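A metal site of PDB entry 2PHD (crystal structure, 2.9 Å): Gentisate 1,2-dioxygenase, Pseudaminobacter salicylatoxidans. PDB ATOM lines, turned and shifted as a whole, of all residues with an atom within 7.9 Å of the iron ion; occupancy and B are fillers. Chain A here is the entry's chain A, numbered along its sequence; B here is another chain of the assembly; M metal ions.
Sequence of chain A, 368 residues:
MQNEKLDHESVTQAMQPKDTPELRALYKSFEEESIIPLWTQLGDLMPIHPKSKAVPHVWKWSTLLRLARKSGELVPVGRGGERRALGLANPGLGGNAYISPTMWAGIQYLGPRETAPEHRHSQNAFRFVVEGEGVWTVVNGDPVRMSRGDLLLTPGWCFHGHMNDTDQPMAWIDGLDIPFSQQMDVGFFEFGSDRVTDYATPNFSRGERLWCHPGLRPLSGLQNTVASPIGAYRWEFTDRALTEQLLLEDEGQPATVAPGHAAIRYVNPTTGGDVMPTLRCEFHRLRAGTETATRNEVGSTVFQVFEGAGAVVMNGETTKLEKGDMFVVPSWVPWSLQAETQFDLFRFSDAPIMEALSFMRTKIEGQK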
ATOM      1  N   GLN A 108     -26.200 -33.073  -8.985  1.00  0.00           N
ATOM      2  CA  GLN A 108     -25.037 -32.440  -9.559  1.00  0.00           C
ATOM      3  C   GLN A 108     -23.808 -33.179  -9.041  1.00  0.00           C
ATOM      4  O   GLN A 108     -23.707 -33.448  -7.837  1.00  0.00           O
ATOM      5  CB  GLN A 108     -25.031 -30.994  -9.123  1.00  0.00           C
ATOM      6  CG  GLN A 108     -23.715 -30.348  -9.151  1.00  0.00           C
ATOM      7  CD  GLN A 108     -23.545 -29.469 -10.359  1.00  0.00           C
ATOM      8  OE1 GLN A 108     -24.363 -28.569 -10.616  1.00  0.00           O
ATOM      9  NE2 GLN A 108     -22.455 -29.724 -11.124  1.00  0.00           N
ATOM     10  N   PRO A 117     -17.613 -20.978 -13.293  1.00  0.00           N
ATOM     11  CA  PRO A 117     -17.552 -19.510 -13.195  1.00  0.00           C
ATOM     12  C   PRO A 117     -18.915 -18.976 -12.734  1.00  0.00           C
ATOM     13  O   PRO A 117     -19.907 -19.730 -12.696  1.00  0.00           O
ATOM     14  CB  PRO A 117     -17.237 -19.075 -14.616  1.00  0.00           C
ATOM     15  CG  PRO A 117     -17.868 -20.149 -15.463  1.00  0.00           C
ATOM     16  CD  PRO A 117     -17.647 -21.432 -14.699  1.00  0.00           C
ATOM     17  N   GLU A 118     -18.947 -17.689 -12.398  1.00  0.00           N
ATOM     18  CA  GLU A 118     -20.112 -17.071 -11.780  1.00  0.00           C
ATOM     19  C   GLU A 118     -21.188 -16.724 -12.790  1.00  0.00           C
ATOM     20  O   GLU A 118     -20.919 -16.126 -13.836  1.00  0.00           O
ATOM     21  CB  GLU A 118     -19.688 -15.819 -11.008  1.00  0.00           C
ATOM     22  CG  GLU A 118     -18.840 -16.113  -9.768  1.00  0.00           C
ATOM     23  CD  GLU A 118     -18.630 -14.876  -8.883  1.00  0.00           C
ATOM     24  OE1 GLU A 118     -19.271 -13.830  -9.142  1.00  0.00           O
ATOM     25  OE2 GLU A 118     -17.821 -14.934  -7.925  1.00  0.00           O
ATOM     26  N   HIS A 119     -22.417 -17.144 -12.505  1.00  0.00           N
ATOM     27  CA  HIS A 119     -23.585 -16.697 -13.266  1.00  0.00           C
ATOM     28  C   HIS A 119     -24.653 -16.143 -12.318  1.00  0.00           C
ATOM     29  O   HIS A 119     -24.453 -16.087 -11.111  1.00  0.00           O
ATOM     30  CB  HIS A 119     -24.085 -17.779 -14.275  1.00  0.00           C
ATOM     31  CG  HIS A 119     -24.696 -19.011 -13.651  1.00  0.00           C
ATOM     32  ND1 HIS A 119     -24.496 -20.272 -14.167  1.00  0.00           N
ATOM     33  CD2 HIS A 119     -25.558 -19.161 -12.610  1.00  0.00           C
ATOM     34  CE1 HIS A 119     -25.186 -21.155 -13.453  1.00  0.00           C
ATOM     35  NE2 HIS A 119     -25.842 -20.515 -12.499  1.00  0.00           N
ATOM     36  N   ARG A 120     -25.804 -15.770 -12.858  1.00  0.00           N
ATOM     37  CA  ARG A 120     -26.845 -15.067 -12.117  1.00  0.00           C
ATOM     38  C   ARG A 120     -28.146 -15.277 -12.905  1.00  0.00           C
ATOM     39  O   ARG A 120     -28.159 -15.057 -14.107  1.00  0.00           O
ATOM     40  CB  ARG A 120     -26.461 -13.600 -12.154  1.00  0.00           C
ATOM     41  CG  ARG A 120     -27.079 -12.688 -11.158  1.00  0.00           C
ATOM     42  CD  ARG A 120     -27.171 -11.374 -11.872  1.00  0.00           C
ATOM     43  NE  ARG A 120     -26.999 -10.223 -10.986  1.00  0.00           N
ATOM     44  CZ  ARG A 120     -26.993  -8.971 -11.412  1.00  0.00           C
ATOM     45  NH1 ARG A 120     -26.836  -7.968 -10.558  1.00  0.00           N
ATOM     46  NH2 ARG A 120     -27.143  -8.710 -12.710  1.00  0.00           N
ATOM     47  N   HIS A 121     -29.205 -15.709 -12.241  1.00  0.00           N
ATOM     48  CA  HIS A 121     -30.478 -15.974 -12.923  1.00  0.00           C
ATOM     49  C   HIS A 121     -31.666 -15.665 -12.027  1.00  0.00           C
ATOM     50  O   HIS A 121     -31.557 -15.787 -10.802  1.00  0.00           O
ATOM     51  CB  HIS A 121     -30.547 -17.429 -13.461  1.00  0.00           C
ATOM     52  CG  HIS A 121     -29.891 -18.469 -12.599  1.00  0.00           C
ATOM     53  ND1 HIS A 121     -30.528 -19.093 -11.544  1.00  0.00           N
ATOM     54  CD2 HIS A 121     -28.654 -19.048 -12.681  1.00  0.00           C
ATOM     55  CE1 HIS A 121     -29.709 -19.992 -10.997  1.00  0.00           C
ATOM     56  NE2 HIS A 121     -28.571 -19.983 -11.676  1.00  0.00           N
ATOM     57  N   GLN A 123     -34.345 -17.329 -11.639  1.00  0.00           N
ATOM     58  CA  GLN A 123     -34.855 -18.559 -11.060  1.00  0.00           C
ATOM     59  C   GLN A 123     -34.186 -18.762  -9.718  1.00  0.00           C
ATOM     60  O   GLN A 123     -32.982 -18.552  -9.586  1.00  0.00           O
ATOM     61  CB  GLN A 123     -34.559 -19.767 -11.947  1.00  0.00           C
ATOM     62  CG  GLN A 123     -35.266 -19.772 -13.293  1.00  0.00           C
ATOM     63  CD  GLN A 123     -34.530 -18.996 -14.391  1.00  0.00           C
ATOM     64  OE1 GLN A 123     -33.627 -18.181 -14.103  1.00  0.00           O
ATOM     65  NE2 GLN A 123     -34.897 -19.249 -15.657  1.00  0.00           N
ATOM     66  N   ALA A 125     -32.845 -20.900  -6.472  1.00  0.00           N
ATOM     67  CA  ALA A 125     -32.120 -22.172  -6.397  1.00  0.00           C
ATOM     68  C   ALA A 125     -31.569 -22.498  -5.007  1.00  0.00           C
ATOM     69  O   ALA A 125     -31.166 -21.599  -4.255  1.00  0.00           O
ATOM     70  CB  ALA A 125     -30.991 -22.158  -7.426  1.00  0.00           C
ATOM     71  N   ARG A 127     -29.043 -25.792  -2.915  1.00  0.00           N
ATOM     72  CA  ARG A 127     -28.165 -26.912  -3.088  1.00  0.00           C
ATOM     73  C   ARG A 127     -28.122 -27.660  -1.786  1.00  0.00           C
ATOM     74  O   ARG A 127     -27.652 -27.122  -0.771  1.00  0.00           O
ATOM     75  CB  ARG A 127     -26.752 -26.407  -3.441  1.00  0.00           C
ATOM     76  CG  ARG A 127     -26.602 -25.787  -4.855  1.00  0.00           C
ATOM     77  CD  ARG A 127     -25.209 -25.215  -5.144  1.00  0.00           C
ATOM     78  NE  ARG A 127     -25.215 -24.553  -6.451  1.00  0.00           N
ATOM     79  CZ  ARG A 127     -24.129 -24.151  -7.126  1.00  0.00           C
ATOM     80  NH1 ARG A 127     -22.900 -24.340  -6.607  1.00  0.00           N
ATOM     81  NH2 ARG A 127     -24.267 -23.558  -8.306  1.00  0.00           N
ATOM     82  N   THR A 154     -28.964 -20.269  -3.242  1.00  0.00           N
ATOM     83  CA  THR A 154     -28.561 -19.224  -4.187  1.00  0.00           C
ATOM     84  C   THR A 154     -29.830 -18.578  -4.750  1.00  0.00           C
ATOM     85  O   THR A 154     -30.300 -18.947  -5.831  1.00  0.00           O
ATOM     86  CB  THR A 154     -27.624 -19.757  -5.263  1.00  0.00           C
ATOM     87  OG1 THR A 154     -28.267 -20.823  -5.960  1.00  0.00           O
ATOM     88  CG2 THR A 154     -26.309 -20.239  -4.653  1.00  0.00           C
ATOM     89  N   CYS A 158     -28.884 -13.673  -7.430  1.00  0.00           N
ATOM     90  CA  CYS A 158     -27.583 -13.627  -6.776  1.00  0.00           C
ATOM     91  C   CYS A 158     -26.486 -14.346  -7.584  1.00  0.00           C
ATOM     92  O   CYS A 158     -26.672 -15.531  -7.984  1.00  0.00           O
ATOM     93  CB  CYS A 158     -27.643 -14.308  -5.399  1.00  0.00           C
ATOM     94  SG  CYS A 158     -28.890 -13.642  -4.264  1.00  0.00           S
ATOM     95  N   PHE A 159     -25.350 -13.663  -7.774  1.00  0.00           N
ATOM     96  CA  PHE A 159     -24.178 -14.274  -8.445  1.00  0.00           C
ATOM     97  C   PHE A 159     -23.732 -15.494  -7.663  1.00  0.00           C
ATOM     98  O   PHE A 159     -23.600 -15.423  -6.440  1.00  0.00           O
ATOM     99  CB  PHE A 159     -23.007 -13.285  -8.645  1.00  0.00           C
ATOM    100  CG  PHE A 159     -23.248 -12.260  -9.751  1.00  0.00           C
ATOM    101  CD1 PHE A 159     -23.632 -10.941  -9.447  1.00  0.00           C
ATOM    102  CD2 PHE A 159     -23.120 -12.606 -11.114  1.00  0.00           C
ATOM    103  CE1 PHE A 159     -23.874  -9.977 -10.480  1.00  0.00           C
ATOM    104  CE2 PHE A 159     -23.352 -11.642 -12.151  1.00  0.00           C
ATOM    105  CZ  PHE A 159     -23.726 -10.341 -11.825  1.00  0.00           C
ATOM    106  N   HIS A 160     -23.544 -16.611  -8.355  1.00  0.00           N
ATOM    107  CA  HIS A 160     -22.960 -17.822  -7.767  1.00  0.00           C
ATOM    108  C   HIS A 160     -22.026 -18.547  -8.739  1.00  0.00           C
ATOM    109  O   HIS A 160     -22.280 -18.623  -9.938  1.00  0.00           O
ATOM    110  CB  HIS A 160     -24.051 -18.778  -7.259  1.00  0.00           C
ATOM    111  CG  HIS A 160     -25.088 -19.127  -8.284  1.00  0.00           C
ATOM    112  ND1 HIS A 160     -26.164 -18.319  -8.554  1.00  0.00           N
ATOM    113  CD2 HIS A 160     -25.192 -20.190  -9.115  1.00  0.00           C
ATOM    114  CE1 HIS A 160     -26.879 -18.868  -9.520  1.00  0.00           C
ATOM    115  NE2 HIS A 160     -26.322 -20.007  -9.878  1.00  0.00           N
ATOM    116  N   GLY A 161     -20.907 -19.028  -8.205  1.00  0.00           N
ATOM    117  CA  GLY A 161     -20.097 -20.054  -8.832  1.00  0.00           C
ATOM    118  C   GLY A 161     -19.516 -20.890  -7.698  1.00  0.00           C
ATOM    119  O   GLY A 161     -19.779 -20.622  -6.502  1.00  0.00           O
ATOM    120  N   HIS A 162     -18.699 -21.885  -8.028  1.00  0.00           N
ATOM    121  CA  HIS A 162     -18.091 -22.754  -7.015  1.00  0.00           C
ATOM    122  C   HIS A 162     -16.688 -23.184  -7.409  1.00  0.00           C
ATOM    123  O   HIS A 162     -16.357 -23.213  -8.588  1.00  0.00           O
ATOM    124  CB  HIS A 162     -18.962 -24.007  -6.744  1.00  0.00           C
ATOM    125  CG  HIS A 162     -19.338 -24.743  -7.993  1.00  0.00           C
ATOM    126  ND1 HIS A 162     -20.561 -24.583  -8.607  1.00  0.00           N
ATOM    127  CD2 HIS A 162     -18.637 -25.606  -8.766  1.00  0.00           C
ATOM    128  CE1 HIS A 162     -20.612 -25.334  -9.701  1.00  0.00           C
ATOM    129  NE2 HIS A 162     -19.445 -25.957  -9.828  1.00  0.00           N
ATOM    130  N   ASP A 174     -29.649 -30.303  -6.753  1.00  0.00           N
ATOM    131  CA  ASP A 174     -29.965 -28.993  -7.287  1.00  0.00           C
ATOM    132  C   ASP A 174     -31.478 -28.861  -7.296  1.00  0.00           C
ATOM    133  O   ASP A 174     -32.154 -29.632  -7.982  1.00  0.00           O
ATOM    134  CB  ASP A 174     -29.487 -28.911  -8.745  1.00  0.00           C
ATOM    135  CG  ASP A 174     -28.239 -28.020  -8.937  1.00  0.00           C
ATOM    136  OD1 ASP A 174     -27.957 -27.123  -8.091  1.00  0.00           O
ATOM    137  OD2 ASP A 174     -27.562 -28.189  -9.993  1.00  0.00           O
ATOM    138  N   LEU A 176     -34.542 -26.080  -8.176  1.00  0.00           N
ATOM    139  CA  LEU A 176     -34.829 -24.816  -8.870  1.00  0.00           C
ATOM    140  C   LEU A 176     -36.296 -24.657  -9.277  1.00  0.00           C
ATOM    141  O   LEU A 176     -37.033 -25.633  -9.417  1.00  0.00           O
ATOM    142  CB  LEU A 176     -33.941 -24.703 -10.119  1.00  0.00           C
ATOM    143  CG  LEU A 176     -32.443 -24.525  -9.846  1.00  0.00           C
ATOM    144  CD1 LEU A 176     -31.714 -25.846  -9.910  1.00  0.00           C
ATOM    145  CD2 LEU A 176     -31.770 -23.515 -10.764  1.00  0.00           C
ATOM    146  N   ILE A 178     -37.120 -23.774 -12.175  1.00  0.00           N
ATOM    147  CA  ILE A 178     -36.920 -23.727 -13.644  1.00  0.00           C
ATOM    148  C   ILE A 178     -38.214 -23.977 -14.414  1.00  0.00           C
ATOM    149  O   ILE A 178     -38.557 -23.185 -15.295  1.00  0.00           O
ATOM    150  CB  ILE A 178     -35.767 -24.715 -14.109  1.00  0.00           C
ATOM    151  CG1 ILE A 178     -34.356 -24.090 -13.949  1.00  0.00           C
ATOM    152  CG2 ILE A 178     -35.986 -25.220 -15.540  1.00  0.00           C
ATOM    153  CD1 ILE A 178     -33.170 -25.060 -14.153  1.00  0.00           C
ATOM    154  N   PHE A 189     -30.998 -14.133 -17.327  1.00  0.00           N
ATOM    155  CA  PHE A 189     -29.706 -14.737 -17.056  1.00  0.00           C
ATOM    156  C   PHE A 189     -28.603 -13.782 -17.432  1.00  0.00           C
ATOM    157  O   PHE A 189     -28.649 -13.185 -18.500  1.00  0.00           O
ATOM    158  CB  PHE A 189     -29.545 -16.018 -17.845  1.00  0.00           C
ATOM    159  CG  PHE A 189     -28.292 -16.790 -17.544  1.00  0.00           C
ATOM    160  CD1 PHE A 189     -27.073 -16.423 -18.129  1.00  0.00           C
ATOM    161  CD2 PHE A 189     -28.310 -17.896 -16.717  1.00  0.00           C
ATOM    162  CE1 PHE A 189     -25.932 -17.132 -17.876  1.00  0.00           C
ATOM    163  CE2 PHE A 189     -27.162 -18.614 -16.473  1.00  0.00           C
ATOM    164  CZ  PHE A 189     -25.982 -18.225 -17.049  1.00  0.00           C
ATOM    165  N   LEU B  38     -28.436 -32.059 -17.773  1.00  0.00           N
ATOM    166  CA  LEU B  38     -28.541 -30.617 -18.019  1.00  0.00           C
ATOM    167  C   LEU B  38     -27.804 -30.179 -19.274  1.00  0.00           C
ATOM    168  O   LEU B  38     -28.275 -29.276 -19.977  1.00  0.00           O
ATOM    169  CB  LEU B  38     -28.029 -29.786 -16.824  1.00  0.00           C
ATOM    170  CG  LEU B  38     -28.227 -28.260 -16.930  1.00  0.00           C
ATOM    171  CD1 LEU B  38     -29.702 -27.861 -17.162  1.00  0.00           C
ATOM    172  CD2 LEU B  38     -27.650 -27.507 -15.732  1.00  0.00           C
ATOM    173  N   MET B  46     -32.824 -21.737 -19.682  1.00  0.00           N
ATOM    174  CA  MET B  46     -32.624 -20.591 -18.785  1.00  0.00           C
ATOM    175  C   MET B  46     -32.174 -19.388 -19.634  1.00  0.00           C
ATOM    176  O   MET B  46     -30.969 -19.118 -19.770  1.00  0.00           O
ATOM    177  CB  MET B  46     -31.612 -20.921 -17.704  1.00  0.00           C
ATOM    178  CG  MET B  46     -32.112 -21.934 -16.731  1.00  0.00           C
ATOM    179  SD  MET B  46     -30.960 -22.056 -15.378  1.00  0.00           S
ATOM    180  CE  MET B  46     -31.597 -20.857 -14.233  1.00  0.00           C
HETATM  181 FE    FE M   1     -27.006 -21.482 -11.293  1.00  0.00          FE
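The backbone carbonyl oxygen (O) of Gln 123 is in hydrogen-bond range of a ring nitrogen (ND1) of His 121, at 3.2 Å. O of Cys 158 is in hydrogen-bond range of ND1 of His 160 (2.9 Å).
Three residues have an atom within 4 Å of the iron ion: His 119, His 121 and His 160.
NE2 of His 119 is bound to the iron ion, at 1.9 Å. NE2 of His 160 is bound to the iron ion, at 2.2 Å. The iron ion is bound by NE2 of His 121, 2.2 Å away.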
